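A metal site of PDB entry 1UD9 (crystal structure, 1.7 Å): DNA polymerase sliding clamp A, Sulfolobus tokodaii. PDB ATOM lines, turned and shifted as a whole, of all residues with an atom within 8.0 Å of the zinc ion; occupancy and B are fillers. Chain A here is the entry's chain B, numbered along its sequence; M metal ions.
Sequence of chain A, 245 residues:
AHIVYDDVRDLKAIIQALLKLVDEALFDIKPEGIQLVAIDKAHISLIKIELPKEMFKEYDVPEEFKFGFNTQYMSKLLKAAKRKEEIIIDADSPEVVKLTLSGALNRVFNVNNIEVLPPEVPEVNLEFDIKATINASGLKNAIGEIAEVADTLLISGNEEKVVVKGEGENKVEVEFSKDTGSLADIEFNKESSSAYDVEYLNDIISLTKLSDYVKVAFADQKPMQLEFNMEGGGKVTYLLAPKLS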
ATOM      1  N   ALA A 150      -6.205  17.210 -24.203  1.00  0.00           N
ATOM      2  CA  ALA A 150      -4.807  16.811 -24.038  1.00  0.00           C
ATOM      3  C   ALA A 150      -4.654  15.801 -22.889  1.00  0.00           C
ATOM      4  O   ALA A 150      -5.565  15.702 -22.073  1.00  0.00           O
ATOM      5  CB  ALA A 150      -3.978  18.079 -23.760  1.00  0.00           C
ATOM      6  N   ASP A 151      -3.552  15.048 -22.829  1.00  0.00           N
ATOM      7  CA  ASP A 151      -3.358  14.095 -21.743  1.00  0.00           C
ATOM      8  C   ASP A 151      -2.530  14.771 -20.670  1.00  0.00           C
ATOM      9  O   ASP A 151      -2.392  14.238 -19.589  1.00  0.00           O
ATOM     10  CB  ASP A 151      -2.575  12.808 -22.130  1.00  0.00           C
ATOM     11  CG  ASP A 151      -2.245  11.861 -20.883  1.00  0.00           C
ATOM     12  OD1 ASP A 151      -1.073  11.452 -20.723  1.00  0.00           O
ATOM     13  OD2 ASP A 151      -3.165  11.493 -20.051  1.00  0.00           O
ATOM     14  N   THR A 152      -1.976  15.927 -21.020  1.00  0.00           N
ATOM     15  CA  THR A 152      -1.056  16.627 -20.118  1.00  0.00           C
ATOM     16  C   THR A 152      -1.346  18.047 -19.866  1.00  0.00           C
ATOM     17  O   THR A 152      -1.776  18.838 -20.760  1.00  0.00           O
ATOM     18  CB  THR A 152       0.328  16.543 -20.648  1.00  0.00           C
ATOM     19  OG1 THR A 152       0.629  15.176 -20.780  1.00  0.00           O
ATOM     20  CG2 THR A 152       1.357  17.214 -19.693  1.00  0.00           C
ATOM     21  N   TYR A 196       2.054  17.578 -15.559  1.00  0.00           N
ATOM     22  CA  TYR A 196       1.333  16.535 -14.822  1.00  0.00           C
ATOM     23  C   TYR A 196       0.287  15.826 -15.734  1.00  0.00           C
ATOM     24  O   TYR A 196      -0.188  16.385 -16.687  1.00  0.00           O
ATOM     25  CB  TYR A 196       0.605  17.190 -13.634  1.00  0.00           C
ATOM     26  CG  TYR A 196       1.493  17.971 -12.694  1.00  0.00           C
ATOM     27  CD1 TYR A 196       1.703  19.344 -12.904  1.00  0.00           C
ATOM     28  CD2 TYR A 196       2.286  17.332 -11.719  1.00  0.00           C
ATOM     29  CE1 TYR A 196       2.702  20.016 -12.186  1.00  0.00           C
ATOM     30  CE2 TYR A 196       3.263  17.985 -10.995  1.00  0.00           C
ATOM     31  CZ  TYR A 196       3.469  19.366 -11.255  1.00  0.00           C
ATOM     32  OH  TYR A 196       4.448  20.008 -10.559  1.00  0.00           O
ATOM     33  N   ASP A 197      -0.134  14.600 -15.363  1.00  0.00           N
ATOM     34  CA  ASP A 197      -1.136  13.846 -16.128  1.00  0.00           C
ATOM     35  C   ASP A 197      -2.473  14.445 -15.748  1.00  0.00           C
ATOM     36  O   ASP A 197      -2.880  14.327 -14.584  1.00  0.00           O
ATOM     37  CB  ASP A 197      -1.125  12.381 -15.670  1.00  0.00           C
ATOM     38  CG  ASP A 197      -2.113  11.537 -16.431  1.00  0.00           C
ATOM     39  OD1 ASP A 197      -3.233  11.999 -16.795  1.00  0.00           O
ATOM     40  OD2 ASP A 197      -1.772  10.389 -16.618  1.00  0.00           O
ATOM     41  N   VAL A 198      -3.161  15.054 -16.692  1.00  0.00           N
ATOM     42  CA  VAL A 198      -4.367  15.758 -16.425  1.00  0.00           C
ATOM     43  C   VAL A 198      -5.517  14.813 -16.088  1.00  0.00           C
ATOM     44  O   VAL A 198      -6.471  15.260 -15.437  1.00  0.00           O
ATOM     45  CB  VAL A 198      -4.740  16.709 -17.583  1.00  0.00           C
ATOM     46  CG1 VAL A 198      -5.315  15.947 -18.803  1.00  0.00           C
ATOM     47  CG2 VAL A 198      -5.705  17.801 -17.062  1.00  0.00           C
ATOM     48  N   GLU A 199      -5.386  13.548 -16.473  1.00  0.00           N
ATOM     49  CA  GLU A 199      -6.435  12.543 -16.154  1.00  0.00           C
ATOM     50  C   GLU A 199      -6.524  12.417 -14.630  1.00  0.00           C
ATOM     51  O   GLU A 199      -7.626  12.270 -14.083  1.00  0.00           O
ATOM     52  CB  GLU A 199      -6.095  11.095 -16.592  1.00  0.00           C
ATOM     53  CG  GLU A 199      -5.597  10.794 -17.989  1.00  0.00           C
ATOM     54  CD  GLU A 199      -5.152   9.316 -18.148  1.00  0.00           C
ATOM     55  OE1 GLU A 199      -4.133   8.884 -17.517  1.00  0.00           O
ATOM     56  OE2 GLU A 199      -5.835   8.581 -18.909  1.00  0.00           O
ATOM     57  N   TYR A 200      -5.380  12.416 -13.961  1.00  0.00           N
ATOM     58  CA  TYR A 200      -5.421  12.288 -12.505  1.00  0.00           C
ATOM     59  C   TYR A 200      -6.068  13.503 -11.877  1.00  0.00           C
ATOM     60  O   TYR A 200      -6.890  13.399 -10.940  1.00  0.00           O
ATOM     61  CB  TYR A 200      -4.024  12.094 -11.901  1.00  0.00           C
ATOM     62  CG  TYR A 200      -3.451  10.743 -12.146  1.00  0.00           C
ATOM     63  CD1 TYR A 200      -3.238  10.276 -13.454  1.00  0.00           C
ATOM     64  CD2 TYR A 200      -3.128   9.909 -11.068  1.00  0.00           C
ATOM     65  CE1 TYR A 200      -2.718   9.006 -13.657  1.00  0.00           C
ATOM     66  CE2 TYR A 200      -2.629   8.649 -11.280  1.00  0.00           C
ATOM     67  CZ  TYR A 200      -2.418   8.213 -12.561  1.00  0.00           C
ATOM     68  OH  TYR A 200      -1.761   7.025 -12.713  1.00  0.00           O
ATOM     69  N   LYS A 243       5.467  14.766 -14.363  1.00  0.00           N
ATOM     70  CA  LYS A 243       5.991  14.161 -15.576  1.00  0.00           C
ATOM     71  C   LYS A 243       7.218  15.046 -15.912  1.00  0.00           C
ATOM     72  O   LYS A 243       7.464  16.058 -15.261  1.00  0.00           O
ATOM     73  CB  LYS A 243       5.029  14.254 -16.731  1.00  0.00           C
ATOM     74  CG  LYS A 243       3.791  13.355 -16.516  1.00  0.00           C
ATOM     75  CD  LYS A 243       4.243  11.892 -16.249  1.00  0.00           C
ATOM     76  CE  LYS A 243       3.106  10.830 -16.404  1.00  0.00           C
ATOM     77  NZ  LYS A 243       2.559  10.790 -17.867  1.00  0.00           N
HETATM   78 ZN    ZN M   1      -2.115   9.930 -18.582  1.00  0.00          ZN
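The backbone carbonyl oxygen (O) of Asp 151 sits at hydrogen-bond distance from the backbone NH (N) of Val 198 (3.1 Å).
Of the 9 residues printed, 3 come within 4 Å of the zinc ion.
The zinc ion is bound by OD2 of Asp 197 (2.0 Å), OD2 of Asp 151 (2.4 Å) and OE1 of Glu 199 (2.5 Å). Slightly farther from the zinc ion lies the side-chain carboxylate (OD1) of Asp 151 (2.8 Å).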
